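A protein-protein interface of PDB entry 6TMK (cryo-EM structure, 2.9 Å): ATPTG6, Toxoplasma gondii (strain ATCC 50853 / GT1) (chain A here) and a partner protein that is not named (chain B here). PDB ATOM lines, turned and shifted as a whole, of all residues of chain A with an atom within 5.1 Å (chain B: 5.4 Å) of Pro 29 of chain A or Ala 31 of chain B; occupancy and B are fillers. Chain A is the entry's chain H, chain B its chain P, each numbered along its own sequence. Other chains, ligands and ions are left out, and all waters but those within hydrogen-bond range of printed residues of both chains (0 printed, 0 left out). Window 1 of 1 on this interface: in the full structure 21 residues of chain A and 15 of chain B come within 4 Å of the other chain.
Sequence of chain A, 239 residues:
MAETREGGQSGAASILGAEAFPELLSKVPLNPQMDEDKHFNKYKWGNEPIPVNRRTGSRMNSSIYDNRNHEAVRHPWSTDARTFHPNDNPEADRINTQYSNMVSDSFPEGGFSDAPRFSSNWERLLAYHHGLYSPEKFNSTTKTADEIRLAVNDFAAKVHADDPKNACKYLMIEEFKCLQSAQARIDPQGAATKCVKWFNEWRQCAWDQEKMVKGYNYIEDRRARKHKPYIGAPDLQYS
The side-chain hydroxyl of Ser 34 of chain B is in hydrogen-bond range of the backbone carbonyl oxygen of Leu 30 of chain A, at 3.3 Å.
The backbone NH (N) of Leu 30 of chain A is in hydrogen-bond range of the side-chain sulfur (SD) of Met 34 of chain A (3.6 Å).
OD2 of Asp 35 of chain A is in hydrogen-bond range of N of Tyr 43 of chain A (3.4 Å).
The backbone carbonyl oxygen (O) of Ala 30 of chain B is in hydrogen-bond range of the side-chain hydroxyl (OG) of Ser 34 of chain B.
Pro 29 of chain A touches Ala 31 of chain B (O to CB, 3.9 Å).
Leu 30 of chain A touches Lys 27 of chain B.
Leu 30 of chain A touches Ala 31 of chain B.
Ser 34 of chain B touches Tyr 43 of chain A (C to OH, 3.9 Å).
Ala 35 of chain B touches Tyr 43 of chain A (CA to OH, 3.6 Å).
CE2 of Tyr 43 of chain A touches CB of Ala 43 of chain B, at 3.96 Å.
Printed residues of chain B within 4 Å of Pro 29 of chain A: Ala 31 (3.9 Å).
Printed residues of chain A within 4 Å of Lys 27 of chain B: Leu 30.
Of chain A, only Pro 29 (3.9 Å) and Leu 30 (3.7 Å) come within 4 Å of Ala 31 of chain B.
Printed residues of chain A within 4 Å of Ala 35 of chain B: Tyr 43 (3.6 Å).
Of the printed residues of chain A, Ala 43 of chain B touches Tyr 43.
The nearest residue of chain B that does not touch Pro 29 of chain A is Ala 43 of chain B (4.7 Å).
Of the 10 printed residues of chain A, 3 touch a printed residue of chain B.
Printed residues of chain A that touch a printed residue of chain B: Pro 29, Leu 30 and Tyr 43.
Hydrophobic or aromatic side chains of chain A that line the printed part of chain B: Leu 30 and Tyr 43.
Along chain A the printed residues that touch a printed residue of chain B span positions 29 to 43.
Of the 13 printed residues of chain B, 5 touch a printed residue of chain A.
Hydrophobic or aromatic side chains of chain B that line the printed part of chain A: Ala 31, Ala 35 and Ala 43.
Among the printed residues, 7 pairs touch across the chains.
Among the printed residues, no Asp or Glu carboxylate lies within 4 Å of a Lys or Arg side-chain nitrogen of the other chain.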
ATOM      1  N   LYS A  27     -25.373  25.113  -3.265  1.00  0.00           N
ATOM      2  CA  LYS A  27     -24.937  25.943  -4.377  1.00  0.00           C
ATOM      3  C   LYS A  27     -23.868  25.220  -5.184  1.00  0.00           C
ATOM      4  O   LYS A  27     -22.685  25.572  -5.129  1.00  0.00           O
ATOM      5  CB  LYS A  27     -24.434  27.289  -3.862  1.00  0.00           C
ATOM      6  CG  LYS A  27     -25.544  28.145  -3.281  1.00  0.00           C
ATOM      7  CD  LYS A  27     -25.013  29.384  -2.586  1.00  0.00           C
ATOM      8  CE  LYS A  27     -24.577  30.437  -3.586  1.00  0.00           C
ATOM      9  NZ  LYS A  27     -23.838  31.556  -2.949  1.00  0.00           N
ATOM     10  N   VAL A  28     -24.286  24.209  -5.934  1.00  0.00           N
ATOM     11  CA  VAL A  28     -23.392  23.369  -6.725  1.00  0.00           C
ATOM     12  C   VAL A  28     -23.526  23.786  -8.184  1.00  0.00           C
ATOM     13  O   VAL A  28     -24.617  23.645  -8.754  1.00  0.00           O
ATOM     14  CB  VAL A  28     -23.724  21.881  -6.559  1.00  0.00           C
ATOM     15  CG1 VAL A  28     -22.674  21.041  -7.235  1.00  0.00           C
ATOM     16  CG2 VAL A  28     -23.835  21.520  -5.107  1.00  0.00           C
ATOM     17  N   PRO A  29     -22.470  24.283  -8.822  1.00  0.00           N
ATOM     18  CA  PRO A  29     -22.564  24.576 -10.255  1.00  0.00           C
ATOM     19  C   PRO A  29     -22.234  23.379 -11.125  1.00  0.00           C
ATOM     20  O   PRO A  29     -21.249  22.676 -10.884  1.00  0.00           O
ATOM     21  CB  PRO A  29     -21.533  25.689 -10.435  1.00  0.00           C
ATOM     22  CG  PRO A  29     -20.488  25.348  -9.445  1.00  0.00           C
ATOM     23  CD  PRO A  29     -21.193  24.750  -8.260  1.00  0.00           C
ATOM     24  N   LEU A  30     -23.055  23.137 -12.147  1.00  0.00           N
ATOM     25  CA  LEU A  30     -22.764  22.063 -13.084  1.00  0.00           C
ATOM     26  C   LEU A  30     -21.631  22.414 -14.032  1.00  0.00           C
ATOM     27  O   LEU A  30     -21.064  21.515 -14.660  1.00  0.00           O
ATOM     28  CB  LEU A  30     -24.019  21.722 -13.881  1.00  0.00           C
ATOM     29  CG  LEU A  30     -25.296  21.585 -13.058  1.00  0.00           C
ATOM     30  CD1 LEU A  30     -26.456  21.279 -13.954  1.00  0.00           C
ATOM     31  CD2 LEU A  30     -25.154  20.521 -11.999  1.00  0.00           C
ATOM     32  N   ASN A  31     -21.292  23.692 -14.150  1.00  0.00           N
ATOM     33  CA  ASN A  31     -20.243  24.140 -15.050  1.00  0.00           C
ATOM     34  C   ASN A  31     -19.850  25.554 -14.658  1.00  0.00           C
ATOM     35  O   ASN A  31     -20.595  26.233 -13.939  1.00  0.00           O
ATOM     36  CB  ASN A  31     -20.699  24.080 -16.515  1.00  0.00           C
ATOM     37  CG  ASN A  31     -22.071  24.663 -16.726  1.00  0.00           C
ATOM     38  OD1 ASN A  31     -22.366  25.772 -16.286  1.00  0.00           O
ATOM     39  ND2 ASN A  31     -22.922  23.916 -17.407  1.00  0.00           N
ATOM     40  N   MET A  34     -22.553  28.211 -15.367  1.00  0.00           N
ATOM     41  CA  MET A  34     -23.584  28.272 -14.339  1.00  0.00           C
ATOM     42  C   MET A  34     -23.052  28.926 -13.072  1.00  0.00           C
ATOM     43  O   MET A  34     -23.760  29.699 -12.415  1.00  0.00           O
ATOM     44  CB  MET A  34     -24.097  26.862 -14.039  1.00  0.00           C
ATOM     45  CG  MET A  34     -24.934  26.744 -12.782  1.00  0.00           C
ATOM     46  SD  MET A  34     -25.924  25.243 -12.697  1.00  0.00           S
ATOM     47  CE  MET A  34     -27.222  25.610 -13.872  1.00  0.00           C
ATOM     48  N   ASP A  35     -21.804  28.625 -12.714  1.00  0.00           N
ATOM     49  CA  ASP A  35     -21.196  29.243 -11.541  1.00  0.00           C
ATOM     50  C   ASP A  35     -21.164  30.760 -11.681  1.00  0.00           C
ATOM     51  O   ASP A  35     -21.578  31.490 -10.774  1.00  0.00           O
ATOM     52  CB  ASP A  35     -19.790  28.683 -11.336  1.00  0.00           C
ATOM     53  CG  ASP A  35     -19.183  29.087 -10.012  1.00  0.00           C
ATOM     54  OD1 ASP A  35     -19.705  28.664  -8.961  1.00  0.00           O
ATOM     55  OD2 ASP A  35     -18.173  29.818 -10.021  1.00  0.00           O
ATOM     56  N   PHE A  40     -22.436  31.515  -7.627  1.00  0.00           N
ATOM     57  CA  PHE A  40     -22.066  30.600  -6.555  1.00  0.00           C
ATOM     58  C   PHE A  40     -20.606  30.777  -6.166  1.00  0.00           C
ATOM     59  O   PHE A  40     -20.253  30.678  -4.984  1.00  0.00           O
ATOM     60  CB  PHE A  40     -22.330  29.157  -6.979  1.00  0.00           C
ATOM     61  CG  PHE A  40     -23.759  28.873  -7.334  1.00  0.00           C
ATOM     62  CD1 PHE A  40     -24.787  29.642  -6.824  1.00  0.00           C
ATOM     63  CD2 PHE A  40     -24.075  27.823  -8.169  1.00  0.00           C
ATOM     64  CE1 PHE A  40     -26.095  29.373  -7.150  1.00  0.00           C
ATOM     65  CE2 PHE A  40     -25.381  27.550  -8.493  1.00  0.00           C
ATOM     66  CZ  PHE A  40     -26.391  28.327  -7.983  1.00  0.00           C
ATOM     67  N   LYS A  42     -17.858  28.955  -6.731  1.00  0.00           N
ATOM     68  CA  LYS A  42     -17.175  27.760  -6.262  1.00  0.00           C
ATOM     69  C   LYS A  42     -16.109  27.276  -7.230  1.00  0.00           C
ATOM     70  O   LYS A  42     -15.507  26.223  -6.993  1.00  0.00           O
ATOM     71  CB  LYS A  42     -18.189  26.642  -6.008  1.00  0.00           C
ATOM     72  CG  LYS A  42     -19.129  26.930  -4.869  1.00  0.00           C
ATOM     73  CD  LYS A  42     -19.567  25.669  -4.171  1.00  0.00           C
ATOM     74  CE  LYS A  42     -20.503  25.984  -3.025  1.00  0.00           C
ATOM     75  NZ  LYS A  42     -21.117  24.763  -2.454  1.00  0.00           N
ATOM     76  N   TYR A  43     -15.860  28.009  -8.310  1.00  0.00           N
ATOM     77  CA  TYR A  43     -14.782  27.708  -9.241  1.00  0.00           C
ATOM     78  C   TYR A  43     -13.647  28.692  -8.986  1.00  0.00           C
ATOM     79  O   TYR A  43     -13.794  29.896  -9.220  1.00  0.00           O
ATOM     80  CB  TYR A  43     -15.263  27.783 -10.686  1.00  0.00           C
ATOM     81  CG  TYR A  43     -15.778  26.472 -11.227  1.00  0.00           C
ATOM     82  CD1 TYR A  43     -15.229  25.902 -12.358  1.00  0.00           C
ATOM     83  CD2 TYR A  43     -16.827  25.815 -10.614  1.00  0.00           C
ATOM     84  CE1 TYR A  43     -15.698  24.707 -12.849  1.00  0.00           C
ATOM     85  CE2 TYR A  43     -17.303  24.625 -11.101  1.00  0.00           C
ATOM     86  CZ  TYR A  43     -16.740  24.079 -12.221  1.00  0.00           C
ATOM     87  OH  TYR A  43     -17.220  22.888 -12.705  1.00  0.00           O
ATOM     88  N   LEU B  26     -28.257  12.477 -11.347  1.00  0.00           N
ATOM     89  CA  LEU B  26     -27.597  12.587 -12.644  1.00  0.00           C
ATOM     90  C   LEU B  26     -26.923  13.944 -12.807  1.00  0.00           C
ATOM     91  O   LEU B  26     -25.782  14.032 -13.287  1.00  0.00           O
ATOM     92  CB  LEU B  26     -28.605  12.348 -13.761  1.00  0.00           C
ATOM     93  CG  LEU B  26     -29.246  10.969 -13.765  1.00  0.00           C
ATOM     94  CD1 LEU B  26     -30.353  10.913 -14.775  1.00  0.00           C
ATOM     95  CD2 LEU B  26     -28.219   9.921 -14.069  1.00  0.00           C
ATOM     96  N   LYS B  27     -27.611  15.013 -12.407  1.00  0.00           N
ATOM     97  CA  LYS B  27     -27.009  16.338 -12.479  1.00  0.00           C
ATOM     98  C   LYS B  27     -25.744  16.412 -11.639  1.00  0.00           C
ATOM     99  O   LYS B  27     -24.747  17.010 -12.054  1.00  0.00           O
ATOM    100  CB  LYS B  27     -28.000  17.396 -12.011  1.00  0.00           C
ATOM    101  CG  LYS B  27     -29.146  17.640 -12.940  1.00  0.00           C
ATOM    102  CD  LYS B  27     -29.965  18.798 -12.461  1.00  0.00           C
ATOM    103  CE  LYS B  27     -31.248  18.908 -13.221  1.00  0.00           C
ATOM    104  NZ  LYS B  27     -32.401  18.816 -12.302  1.00  0.00           N
ATOM    105  N   LEU B  28     -25.766  15.806 -10.453  1.00  0.00           N
ATOM    106  CA  LEU B  28     -24.607  15.879  -9.573  1.00  0.00           C
ATOM    107  C   LEU B  28     -23.442  15.058 -10.106  1.00  0.00           C
ATOM    108  O   LEU B  28     -22.284  15.451  -9.942  1.00  0.00           O
ATOM    109  CB  LEU B  28     -24.987  15.408  -8.177  1.00  0.00           C
ATOM    110  CG  LEU B  28     -25.997  16.297  -7.464  1.00  0.00           C
ATOM    111  CD1 LEU B  28     -26.604  15.578  -6.294  1.00  0.00           C
ATOM    112  CD2 LEU B  28     -25.338  17.564  -7.013  1.00  0.00           C
ATOM    113  N   LEU B  29     -23.724  13.934 -10.759  1.00  0.00           N
ATOM    114  CA  LEU B  29     -22.659  13.182 -11.412  1.00  0.00           C
ATOM    115  C   LEU B  29     -22.014  14.003 -12.521  1.00  0.00           C
ATOM    116  O   LEU B  29     -20.779  14.069 -12.635  1.00  0.00           O
ATOM    117  CB  LEU B  29     -23.220  11.883 -11.978  1.00  0.00           C
ATOM    118  CG  LEU B  29     -23.704  10.831 -10.987  1.00  0.00           C
ATOM    119  CD1 LEU B  29     -24.398   9.711 -11.725  1.00  0.00           C
ATOM    120  CD2 LEU B  29     -22.556  10.294 -10.183  1.00  0.00           C
ATOM    121  N   ALA B  30     -22.840  14.631 -13.356  1.00  0.00           N
ATOM    122  CA  ALA B  30     -22.307  15.499 -14.398  1.00  0.00           C
ATOM    123  C   ALA B  30     -21.465  16.623 -13.809  1.00  0.00           C
ATOM    124  O   ALA B  30     -20.403  16.965 -14.346  1.00  0.00           O
ATOM    125  CB  ALA B  30     -23.451  16.066 -15.231  1.00  0.00           C
ATOM    126  N   ALA B  31     -21.920  17.205 -12.699  1.00  0.00           N
ATOM    127  CA  ALA B  31     -21.172  18.281 -12.061  1.00  0.00           C
ATOM    128  C   ALA B  31     -19.835  17.789 -11.531  1.00  0.00           C
ATOM    129  O   ALA B  31     -18.822  18.486 -11.642  1.00  0.00           O
ATOM    130  CB  ALA B  31     -21.999  18.893 -10.938  1.00  0.00           C
ATOM    131  N   TYR B  32     -19.818  16.599 -10.935  1.00  0.00           N
ATOM    132  CA  TYR B  32     -18.569  16.023 -10.455  1.00  0.00           C
ATOM    133  C   TYR B  32     -17.580  15.850 -11.596  1.00  0.00           C
ATOM    134  O   TYR B  32     -16.401  16.201 -11.472  1.00  0.00           O
ATOM    135  CB  TYR B  32     -18.852  14.688  -9.771  1.00  0.00           C
ATOM    136  CG  TYR B  32     -17.730  14.176  -8.909  1.00  0.00           C
ATOM    137  CD1 TYR B  32     -17.635  14.533  -7.578  1.00  0.00           C
ATOM    138  CD2 TYR B  32     -16.776  13.317  -9.421  1.00  0.00           C
ATOM    139  CE1 TYR B  32     -16.614  14.063  -6.788  1.00  0.00           C
ATOM    140  CE2 TYR B  32     -15.755  12.843  -8.639  1.00  0.00           C
ATOM    141  CZ  TYR B  32     -15.680  13.215  -7.322  1.00  0.00           C
ATOM    142  OH  TYR B  32     -14.660  12.742  -6.534  1.00  0.00           O
ATOM    143  N   ASP B  33     -18.047  15.316 -12.724  1.00  0.00           N
ATOM    144  CA  ASP B  33     -17.157  15.121 -13.864  1.00  0.00           C
ATOM    145  C   ASP B  33     -16.628  16.451 -14.394  1.00  0.00           C
ATOM    146  O   ASP B  33     -15.432  16.580 -14.697  1.00  0.00           O
ATOM    147  CB  ASP B  33     -17.888  14.353 -14.960  1.00  0.00           C
ATOM    148  CG  ASP B  33     -18.186  12.920 -14.568  1.00  0.00           C
ATOM    149  OD1 ASP B  33     -17.442  12.361 -13.735  1.00  0.00           O
ATOM    150  OD2 ASP B  33     -19.162  12.348 -15.100  1.00  0.00           O
ATOM    151  N   SER B  34     -17.496  17.456 -14.506  1.00  0.00           N
ATOM    152  CA  SER B  34     -17.059  18.758 -15.000  1.00  0.00           C
ATOM    153  C   SER B  34     -16.034  19.386 -14.066  1.00  0.00           C
ATOM    154  O   SER B  34     -15.015  19.925 -14.516  1.00  0.00           O
ATOM    155  CB  SER B  34     -18.259  19.685 -15.177  1.00  0.00           C
ATOM    156  OG  SER B  34     -19.273  19.076 -15.954  1.00  0.00           O
ATOM    157  N   ALA B  35     -16.293  19.338 -12.761  1.00  0.00           N
ATOM    158  CA  ALA B  35     -15.367  19.910 -11.794  1.00  0.00           C
ATOM    159  C   ALA B  35     -14.044  19.164 -11.779  1.00  0.00           C
ATOM    160  O   ALA B  35     -12.999  19.774 -11.543  1.00  0.00           O
ATOM    161  CB  ALA B  35     -15.995  19.907 -10.408  1.00  0.00           C
ATOM    162  N   ALA B  36     -14.063  17.856 -12.016  1.00  0.00           N
ATOM    163  CA  ALA B  36     -12.810  17.122 -12.136  1.00  0.00           C
ATOM    164  C   ALA B  36     -12.027  17.585 -13.352  1.00  0.00           C
ATOM    165  O   ALA B  36     -10.812  17.792 -13.274  1.00  0.00           O
ATOM    166  CB  ALA B  36     -13.082  15.628 -12.225  1.00  0.00           C
ATOM    167  N   ALA B  43     -15.929  22.339  -5.588  1.00  0.00           N
ATOM    168  CA  ALA B  43     -17.165  22.045  -6.297  1.00  0.00           C
ATOM    169  C   ALA B  43     -17.454  20.553  -6.298  1.00  0.00           C
ATOM    170  O   ALA B  43     -18.599  20.134  -6.082  1.00  0.00           O
ATOM    171  CB  ALA B  43     -17.084  22.571  -7.724  1.00  0.00           C
ATOM    172  N   ALA B  47     -20.594  18.496  -4.678  1.00  0.00           N
ATOM    173  CA  ALA B  47     -21.406  17.560  -5.442  1.00  0.00           C
ATOM    174  C   ALA B  47     -21.505  16.216  -4.736  1.00  0.00           C
ATOM    175  O   ALA B  47     -22.588  15.629  -4.650  1.00  0.00           O
ATOM    176  CB  ALA B  47     -20.817  17.388  -6.837  1.00  0.00           C
